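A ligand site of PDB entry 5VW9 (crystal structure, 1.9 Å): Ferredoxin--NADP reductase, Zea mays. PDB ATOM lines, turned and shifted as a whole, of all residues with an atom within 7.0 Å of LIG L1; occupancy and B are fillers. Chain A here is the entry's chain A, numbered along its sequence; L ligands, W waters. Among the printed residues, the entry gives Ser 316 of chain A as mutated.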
ATOM      1  N   SER A  71      20.090  -4.922   0.468  1.00  0.00           N
ATOM      2  CA  SER A  71      19.473  -5.304  -0.791  1.00  0.00           C
ATOM      3  C   SER A  71      20.515  -5.459  -1.880  1.00  0.00           C
ATOM      4  O   SER A  71      21.558  -4.800  -1.859  1.00  0.00           O
ATOM      5  CB  SER A  71      18.459  -4.211  -1.220  1.00  0.00           C
ATOM      6  OG  SER A  71      17.350  -4.220  -0.336  1.00  0.00           O
ATOM      7  N   LEU A  92      15.417  -3.520  -7.010  1.00  0.00           N
ATOM      8  CA  LEU A  92      16.016  -3.952  -5.751  1.00  0.00           C
ATOM      9  C   LEU A  92      15.316  -5.174  -5.148  1.00  0.00           C
ATOM     10  O   LEU A  92      14.081  -5.291  -5.197  1.00  0.00           O
ATOM     11  CB  LEU A  92      15.991  -2.796  -4.732  1.00  0.00           C
ATOM     12  CG  LEU A  92      16.863  -1.596  -5.080  1.00  0.00           C
ATOM     13  CD1 LEU A  92      16.528  -0.419  -4.130  1.00  0.00           C
ATOM     14  CD2 LEU A  92      18.342  -1.909  -5.047  1.00  0.00           C
ATOM     15  N   TYR A  93      16.103  -6.047  -4.515  1.00  0.00           N
ATOM     16  CA  TYR A  93      15.573  -7.216  -3.806  1.00  0.00           C
ATOM     17  C   TYR A  93      16.237  -7.332  -2.456  1.00  0.00           C
ATOM     18  O   TYR A  93      17.475  -7.286  -2.358  1.00  0.00           O
ATOM     19  CB  TYR A  93      15.784  -8.496  -4.633  1.00  0.00           C
ATOM     20  CG  TYR A  93      14.945  -8.429  -5.857  1.00  0.00           C
ATOM     21  CD1 TYR A  93      13.599  -8.728  -5.789  1.00  0.00           C
ATOM     22  CD2 TYR A  93      15.454  -7.956  -7.040  1.00  0.00           C
ATOM     23  CE1 TYR A  93      12.779  -8.604  -6.900  1.00  0.00           C
ATOM     24  CE2 TYR A  93      14.649  -7.813  -8.172  1.00  0.00           C
ATOM     25  CZ  TYR A  93      13.311  -8.151  -8.081  1.00  0.00           C
ATOM     26  OH  TYR A  93      12.463  -8.014  -9.150  1.00  0.00           O
ATOM     27  N   SER A  94      15.440  -7.521  -1.418  1.00  0.00           N
ATOM     28  CA  SER A  94      15.963  -7.685  -0.074  1.00  0.00           C
ATOM     29  C   SER A  94      16.723  -8.991   0.028  1.00  0.00           C
ATOM     30  O   SER A  94      16.178 -10.055  -0.262  1.00  0.00           O
ATOM     31  CB  SER A  94      14.823  -7.703   0.936  1.00  0.00           C
ATOM     32  OG  SER A  94      14.003  -6.597   0.743  1.00  0.00           O
ATOM     33  N   ILE A  95      17.964  -8.938   0.491  1.00  0.00           N
ATOM     34  CA  ILE A  95      18.732 -10.177   0.609  1.00  0.00           C
ATOM     35  C   ILE A  95      18.144 -11.007   1.756  1.00  0.00           C
ATOM     36  O   ILE A  95      17.895 -10.503   2.852  1.00  0.00           O
ATOM     37  CB  ILE A  95      20.214  -9.867   0.824  1.00  0.00           C
ATOM     38  CG1 ILE A  95      20.750  -9.066  -0.383  1.00  0.00           C
ATOM     39  CG2 ILE A  95      20.970 -11.131   1.048  1.00  0.00           C
ATOM     40  CD1 ILE A  95      22.068  -8.387  -0.205  1.00  0.00           C
ATOM     41  N   CYS A 112      14.340 -13.638  -2.286  1.00  0.00           N
ATOM     42  CA  CYS A 112      13.009 -14.173  -2.012  1.00  0.00           C
ATOM     43  C   CYS A 112      12.089 -13.346  -2.891  1.00  0.00           C
ATOM     44  O   CYS A 112      11.789 -12.203  -2.560  1.00  0.00           O
ATOM     45  CB  CYS A 112      12.668 -14.041  -0.530  1.00  0.00           C
ATOM     46  SG  CYS A 112      11.006 -14.561  -0.104  1.00  0.00           S
ATOM     47  N   THR A 173       5.218  -8.769   5.856  1.00  0.00           N
ATOM     48  CA  THR A 173       4.219  -9.336   4.980  1.00  0.00           C
ATOM     49  C   THR A 173       4.919  -9.895   3.744  1.00  0.00           C
ATOM     50  O   THR A 173       5.801  -9.237   3.175  1.00  0.00           O
ATOM     51  CB  THR A 173       3.166  -8.288   4.559  1.00  0.00           C
ATOM     52  OG1 THR A 173       3.815  -7.057   4.194  1.00  0.00           O
ATOM     53  CG2 THR A 173       2.188  -8.033   5.702  1.00  0.00           C
ATOM     54  N   GLY A 174       4.505 -11.085   3.337  1.00  0.00           N
ATOM     55  CA  GLY A 174       5.049 -11.740   2.158  1.00  0.00           C
ATOM     56  C   GLY A 174       6.564 -11.773   2.132  1.00  0.00           C
ATOM     57  O   GLY A 174       7.237 -12.126   3.110  1.00  0.00           O
ATOM     58  N   THR A 175       7.130 -11.360   0.993  1.00  0.00           N
ATOM     59  CA  THR A 175       8.582 -11.383   0.807  1.00  0.00           C
ATOM     60  C   THR A 175       9.295 -10.411   1.733  1.00  0.00           C
ATOM     61  O   THR A 175      10.529 -10.411   1.768  1.00  0.00           O
ATOM     62  CB  THR A 175       8.913 -11.030  -0.651  1.00  0.00           C
ATOM     63  OG1 THR A 175       8.238  -9.817  -0.998  1.00  0.00           O
ATOM     64  CG2 THR A 175       8.421 -12.150  -1.574  1.00  0.00           C
ATOM     65  N   GLY A 176       8.562  -9.583   2.462  1.00  0.00           N
ATOM     66  CA  GLY A 176       9.173  -8.778   3.504  1.00  0.00           C
ATOM     67  C   GLY A 176       9.856  -9.597   4.577  1.00  0.00           C
ATOM     68  O   GLY A 176      10.621  -9.041   5.363  1.00  0.00           O
ATOM     69  N   VAL A 177       9.605 -10.918   4.621  1.00  0.00           N
ATOM     70  CA  VAL A 177      10.292 -11.765   5.570  1.00  0.00           C
ATOM     71  C   VAL A 177      11.792 -11.889   5.280  1.00  0.00           C
ATOM     72  O   VAL A 177      12.549 -12.297   6.159  1.00  0.00           O
ATOM     73  CB  VAL A 177       9.666 -13.170   5.590  1.00  0.00           C
ATOM     74  CG1 VAL A 177      10.037 -13.982   4.325  1.00  0.00           C
ATOM     75  CG2 VAL A 177      10.087 -13.913   6.838  1.00  0.00           C
ATOM     76  N   ALA A 178      12.235 -11.543   4.060  1.00  0.00           N
ATOM     77  CA  ALA A 178      13.625 -11.764   3.631  1.00  0.00           C
ATOM     78  C   ALA A 178      14.709 -11.315   4.615  1.00  0.00           C
ATOM     79  O   ALA A 178      15.552 -12.140   5.003  1.00  0.00           O
ATOM     80  CB  ALA A 178      13.850 -11.075   2.289  1.00  0.00           C
ATOM     81  N   PRO A 179      14.770 -10.044   5.026  1.00  0.00           N
ATOM     82  CA  PRO A 179      15.829  -9.645   5.979  1.00  0.00           C
ATOM     83  C   PRO A 179      15.780 -10.416   7.274  1.00  0.00           C
ATOM     84  O   PRO A 179      16.822 -10.689   7.888  1.00  0.00           O
ATOM     85  CB  PRO A 179      15.553  -8.161   6.230  1.00  0.00           C
ATOM     86  CG  PRO A 179      14.050  -7.992   5.914  1.00  0.00           C
ATOM     87  CD  PRO A 179      13.891  -8.885   4.706  1.00  0.00           C
ATOM     88  N   PHE A 273       9.798  -3.241  10.031  1.00  0.00           N
ATOM     89  CA  PHE A 273       8.638  -3.416   9.161  1.00  0.00           C
ATOM     90  C   PHE A 273       9.144  -3.597   7.746  1.00  0.00           C
ATOM     91  O   PHE A 273       9.902  -2.755   7.250  1.00  0.00           O
ATOM     92  CB  PHE A 273       7.682  -2.221   9.209  1.00  0.00           C
ATOM     93  CG  PHE A 273       7.183  -1.891  10.574  1.00  0.00           C
ATOM     94  CD1 PHE A 273       7.888  -1.013  11.374  1.00  0.00           C
ATOM     95  CD2 PHE A 273       6.021  -2.450  11.049  1.00  0.00           C
ATOM     96  CE1 PHE A 273       7.453  -0.706  12.621  1.00  0.00           C
ATOM     97  CE2 PHE A 273       5.567  -2.140  12.320  1.00  0.00           C
ATOM     98  CZ  PHE A 273       6.280  -1.272  13.101  1.00  0.00           C
ATOM     99  N   CYS A 274       8.752  -4.688   7.113  1.00  0.00           N
ATOM    100  CA  CYS A 274       9.273  -4.993   5.798  1.00  0.00           C
ATOM    101  C   CYS A 274       8.215  -5.702   4.966  1.00  0.00           C
ATOM    102  O   CYS A 274       7.528  -6.614   5.438  1.00  0.00           O
ATOM    103  CB  CYS A 274      10.556  -5.828   5.898  1.00  0.00           C
ATOM    104  SG  CYS A 274      11.469  -5.971   4.275  1.00  0.00           S
ATOM    105  N   GLY A 275       8.103  -5.274   3.717  1.00  0.00           N
ATOM    106  CA  GLY A 275       7.146  -5.863   2.821  1.00  0.00           C
ATOM    107  C   GLY A 275       6.220  -4.841   2.193  1.00  0.00           C
ATOM    108  O   GLY A 275       6.683  -3.811   1.707  1.00  0.00           O
ATOM    109  N   LEU A 276       4.916  -5.124   2.257  1.00  0.00           N
ATOM    110  CA  LEU A 276       3.896  -4.300   1.608  1.00  0.00           C
ATOM    111  C   LEU A 276       3.704  -2.965   2.329  1.00  0.00           C
ATOM    112  O   LEU A 276       3.439  -2.947   3.536  1.00  0.00           O
ATOM    113  CB  LEU A 276       2.571  -5.049   1.605  1.00  0.00           C
ATOM    114  CG  LEU A 276       2.475  -6.406   0.928  1.00  0.00           C
ATOM    115  CD1 LEU A 276       1.085  -7.014   1.185  1.00  0.00           C
ATOM    116  CD2 LEU A 276       2.763  -6.271  -0.566  1.00  0.00           C
ATOM    117  N   LYS A 277       3.782  -1.857   1.594  1.00  0.00           N
ATOM    118  CA  LYS A 277       3.544  -0.557   2.212  1.00  0.00           C
ATOM    119  C   LYS A 277       2.126  -0.484   2.752  1.00  0.00           C
ATOM    120  O   LYS A 277       1.871   0.253   3.705  1.00  0.00           O
ATOM    121  CB  LYS A 277       3.797   0.593   1.230  1.00  0.00           C
ATOM    122  CG  LYS A 277       2.954   0.560  -0.033  1.00  0.00           C
ATOM    123  CD  LYS A 277       3.138   1.819  -0.858  1.00  0.00           C
ATOM    124  CE  LYS A 277       2.352   1.744  -2.177  1.00  0.00           C
ATOM    125  NZ  LYS A 277       2.281   3.053  -2.897  1.00  0.00           N
ATOM    126  N   VAL A 313      11.970   0.817   8.949  1.00  0.00           N
ATOM    127  CA  VAL A 313      10.922   0.572   7.962  1.00  0.00           C
ATOM    128  C   VAL A 313      11.533   0.459   6.559  1.00  0.00           C
ATOM    129  O   VAL A 313      12.258   1.369   6.133  1.00  0.00           O
ATOM    130  CB  VAL A 313       9.856   1.685   7.960  1.00  0.00           C
ATOM    131  CG1 VAL A 313       8.785   1.433   6.859  1.00  0.00           C
ATOM    132  CG2 VAL A 313       9.166   1.759   9.301  1.00  0.00           C
ATOM    133  N   GLU A 314      11.201  -0.608   5.831  1.00  0.00           N
ATOM    134  CA  GLU A 314      11.527  -0.681   4.404  1.00  0.00           C
ATOM    135  C   GLU A 314      10.377  -1.413   3.725  1.00  0.00           C
ATOM    136  O   GLU A 314      10.292  -2.647   3.747  1.00  0.00           O
ATOM    137  CB  GLU A 314      12.891  -1.351   4.137  1.00  0.00           C
ATOM    138  CG  GLU A 314      13.546  -0.815   2.844  1.00  0.00           C
ATOM    139  CD  GLU A 314      15.070  -0.841   2.852  1.00  0.00           C
ATOM    140  OE1 GLU A 314      15.650  -1.923   3.083  1.00  0.00           O
ATOM    141  OE2 GLU A 314      15.682   0.220   2.604  1.00  0.00           O
ATOM    142  N   VAL A 315       9.455  -0.627   3.147  1.00  0.00           N
ATOM    143  CA  VAL A 315       8.274  -1.165   2.482  1.00  0.00           C
ATOM    144  C   VAL A 315       8.110  -0.485   1.131  1.00  0.00           C
ATOM    145  O   VAL A 315       8.685   0.577   0.863  1.00  0.00           O
ATOM    146  CB  VAL A 315       7.000  -0.955   3.327  1.00  0.00           C
ATOM    147  CG1 VAL A 315       7.110  -1.665   4.693  1.00  0.00           C
ATOM    148  CG2 VAL A 315       6.716   0.528   3.537  1.00  0.00           C
ATOM    149  N   SER A 316       7.303  -1.113   0.280  1.00  0.00           N
ATOM    150  CA  SER A 316       6.981  -0.540  -1.036  1.00  0.00           C
ATOM    151  C   SER A 316       5.683  -1.137  -1.583  1.00  0.00           C
ATOM    152  O   SER A 316       5.098  -2.071  -1.027  1.00  0.00           O
ATOM    153  CB  SER A 316       8.108  -0.779  -2.029  1.00  0.00           C
ATOM    154  OG  SER A 316       8.116  -2.142  -2.417  1.00  0.00           O
ATOM    155  OXT SER A 316       5.195  -0.679  -2.616  1.00  0.00           O
HETATM  156  N1  LIG L   1       9.592  -3.383  -0.814  1.00  0.00           N
HETATM  157  C1  LIG L   1       9.497  -4.723  -0.658  1.00  0.00           C
HETATM  158  C2  LIG L   1      10.335  -5.400   0.215  1.00  0.00           C
HETATM  159  C3  LIG L   1      11.294  -4.704   0.936  1.00  0.00           C
HETATM  160  C4  LIG L   1      11.389  -3.334   0.738  1.00  0.00           C
HETATM  161  C5  LIG L   1      10.523  -2.696  -0.131  1.00  0.00           C
HETATM  162  C6  LIG L   1      10.195  -6.892   0.346  1.00  0.00           C
HETATM  163  O1  LIG L   1       9.130  -7.413   0.054  1.00  0.00           O
HETATM  164  N2  LIG L   1      11.225  -7.624   0.773  1.00  0.00           N
HETATM  165  P1  LG2 L   2       7.985  -4.538 -13.585  1.00  0.00           P
HETATM  166  O1  LG2 L   2       8.345  -4.974 -15.000  1.00  0.00           O
HETATM  167  O2  LG2 L   2       8.743  -3.375 -12.990  1.00  0.00           O
HETATM  168  O3  LG2 L   2       6.400  -4.234 -13.587  1.00  0.00           O
HETATM  169  C1  LG2 L   2       5.838  -3.568 -12.453  1.00  0.00           C
HETATM  170  C2  LG2 L   2       4.409  -4.042 -12.322  1.00  0.00           C
HETATM  171  O4  LG2 L   2       3.635  -3.595 -13.418  1.00  0.00           O
HETATM  172  C3  LG2 L   2       4.316  -5.554 -12.322  1.00  0.00           C
HETATM  173  O5  LG2 L   2       3.479  -5.894 -11.230  1.00  0.00           O
HETATM  174  C4  LG2 L   2       3.707  -5.889 -13.684  1.00  0.00           C
HETATM  175  O6  LG2 L   2       2.933  -7.084 -13.718  1.00  0.00           O
HETATM  176  C5  LG2 L   2       2.848  -4.673 -13.930  1.00  0.00           C
HETATM  177  N1  LG2 L   2       2.585  -4.326 -15.328  1.00  0.00           N
HETATM  178  C6  LG2 L   2       3.485  -4.177 -16.308  1.00  0.00           C
HETATM  179  N2  LG2 L   2       2.876  -3.817 -17.446  1.00  0.00           N
HETATM  180  C7  LG2 L   2       1.569  -3.733 -17.178  1.00  0.00           C
HETATM  181  C8  LG2 L   2       0.345  -3.380 -17.915  1.00  0.00           C
HETATM  182  N3  LG2 L   2       0.398  -3.040 -19.206  1.00  0.00           N
HETATM  183  N4  LG2 L   2      -0.824  -3.411 -17.254  1.00  0.00           N
HETATM  184  C9  LG2 L   2      -0.912  -3.724 -15.965  1.00  0.00           C
HETATM  185  N5  LG2 L   2       0.148  -4.054 -15.223  1.00  0.00           N
HETATM  186  C10 LG2 L   2       1.379  -4.049 -15.774  1.00  0.00           C
HETATM  187  N6  LG2 L   2      10.144  -7.685  -4.412  1.00  0.00           N
HETATM  188  C11 LG2 L   2      10.260  -9.004  -4.100  1.00  0.00           C
HETATM  189  O7  LG2 L   2       9.534  -9.834  -4.702  1.00  0.00           O
HETATM  190  N7  LG2 L   2      11.120  -9.426  -3.143  1.00  0.00           N
HETATM  191  C12 LG2 L   2      11.927  -8.586  -2.437  1.00  0.00           C
HETATM  192  O8  LG2 L   2      12.731  -8.992  -1.571  1.00  0.00           O
HETATM  193  C13 LG2 L   2      11.850  -7.144  -2.723  1.00  0.00           C
HETATM  194  N8  LG2 L   2      12.612  -6.231  -2.074  1.00  0.00           N
HETATM  195  C14 LG2 L   2      12.581  -4.936  -2.436  1.00  0.00           C
HETATM  196  C15 LG2 L   2      13.375  -4.022  -1.753  1.00  0.00           C
HETATM  197  C16 LG2 L   2      13.257  -2.665  -2.011  1.00  0.00           C
HETATM  198  C17 LG2 L   2      14.115  -1.679  -1.232  1.00  0.00           C
HETATM  199  C18 LG2 L   2      12.302  -2.188  -3.025  1.00  0.00           C
HETATM  200  C19 LG2 L   2      12.150  -0.724  -3.349  1.00  0.00           C
HETATM  201  C20 LG2 L   2      11.539  -3.098  -3.735  1.00  0.00           C
HETATM  202  C21 LG2 L   2      11.650  -4.464  -3.486  1.00  0.00           C
HETATM  203  N9  LG2 L   2      10.832  -5.399  -4.152  1.00  0.00           N
HETATM  204  C22 LG2 L   2      10.910  -6.746  -3.781  1.00  0.00           C
HETATM  205  C23 LG2 L   2      10.116  -5.081  -5.398  1.00  0.00           C
HETATM  206  C24 LG2 L   2      11.035  -5.287  -6.607  1.00  0.00           C
HETATM  207  O9  LG2 L   2      12.084  -4.322  -6.568  1.00  0.00           O
HETATM  208  C25 LG2 L   2      10.281  -5.122  -7.928  1.00  0.00           C
HETATM  209  O10 LG2 L   2       9.661  -3.827  -8.031  1.00  0.00           O
HETATM  210  C26 LG2 L   2       9.227  -6.200  -8.156  1.00  0.00           C
HETATM  211  O11 LG2 L   2       9.856  -7.481  -8.181  1.00  0.00           O
HETATM  212  C27 LG2 L   2       8.566  -6.033  -9.505  1.00  0.00           C
HETATM  213  O12 LG2 L   2       9.557  -5.781 -10.512  1.00  0.00           O
HETATM  214  P2  LG2 L   2       9.368  -6.434 -11.979  1.00  0.00           P
HETATM  215  O13 LG2 L   2      10.587  -6.026 -12.814  1.00  0.00           O
HETATM  216  O14 LG2 L   2       9.025  -7.896 -11.796  1.00  0.00           O
HETATM  217  O15 LG2 L   2       8.037  -5.747 -12.538  1.00  0.00           O
HETATM  218  O   HOH W   1       6.465  -6.961  -0.526  1.00  0.00           O
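O of Gly 176 lies close to SG of Cys 274 (3.4 Å).
The backbone NH (N) of Ser 316 sits at hydrogen-bond distance from the backbone carbonyl oxygen (O) of Gly 275 (3.1 Å).
The backbone carbonyl oxygen (O) of Phe 273 sits at hydrogen-bond distance from the backbone NH (N) of Glu 314, at 2.9 Å.
The backbone NH (N) of Gly 275 is in hydrogen-bond range of the backbone carbonyl oxygen (O) of Glu 314 (3.4 Å).
N of Thr 173 sits at hydrogen-bond distance from O of Cys 274, 3.2 Å away.
O of Ser 316 lies within hydrogen-bond range of N of Lys 277 (2.9 Å).
The side-chain sulfur of Cys 274 lies close to the backbone carbonyl oxygen of Glu 314 (3.6 Å).
Cys 274 touches LIG L1.
Gly 275 touches LIG L1 (CA to O1, 3.7 Å).
Glu 314 touches LIG L1 (O to C4, 3.3 Å).
C of Val 315 touches C5 of LIG L1, at 3.5 Å.
Within 4 Å of LIG L1: Ser 94, Thr 175, Gly 176, Cys 274, Gly 275, Glu 314, Val 315 and Ser 316.
The nearest printed residue that does not touch LIG L1 is Ala 178 (4.6 Å).
O8 of LG2 L2 sits at hydrogen-bond distance from N2 of LIG L1 (3.1 Å).
N of Gly 176 lies within hydrogen-bond range of O1 of LIG L1 (3.3 Å).
OG of Ser 94 lies within hydrogen-bond range of N2 of LIG L1 (3.0 Å).
The backbone NH of Ser 316 lies close to a nitrogen (N1) of LIG L1 (3.4 Å).
O9 of LG2 L2 sits at hydrogen-bond distance from N of Leu 92, 3.5 Å away.
The backbone carbonyl oxygen (O) of Cys 112 lies within hydrogen-bond range of a nitrogen (N7) of LG2 L2 (2.9 Å).
A nitrogen (N1) of LIG L1 is in hydrogen-bond range of the side-chain hydroxyl (OG) of Ser 316.
An oxygen (O9) of LG2 L2 sits at hydrogen-bond distance from the backbone carbonyl oxygen (O) of Leu 92 (2.6 Å).
An oxygen (O1) of LIG L1 sits at hydrogen-bond distance from the side-chain hydroxyl of Thr 175 (2.8 Å).
The side-chain hydroxyl of Ser 94 is in hydrogen-bond range of a nitrogen (N8) of LG2 L2 (3.2 Å).
OH of Tyr 93 is in hydrogen-bond range of O11 of LG2 L2 (2.8 Å).
N of Ser 94 lies within hydrogen-bond range of O8 of LG2 L2, 3.1 Å away.
The backbone carbonyl oxygen (O) of Thr 175 lies within hydrogen-bond range of a nitrogen (N2) of LIG L1, 3.0 Å away.
Water W1 bridges O1 of LIG L1 (2.8 Å) and OG1 of Thr 175 (3.4 Å).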
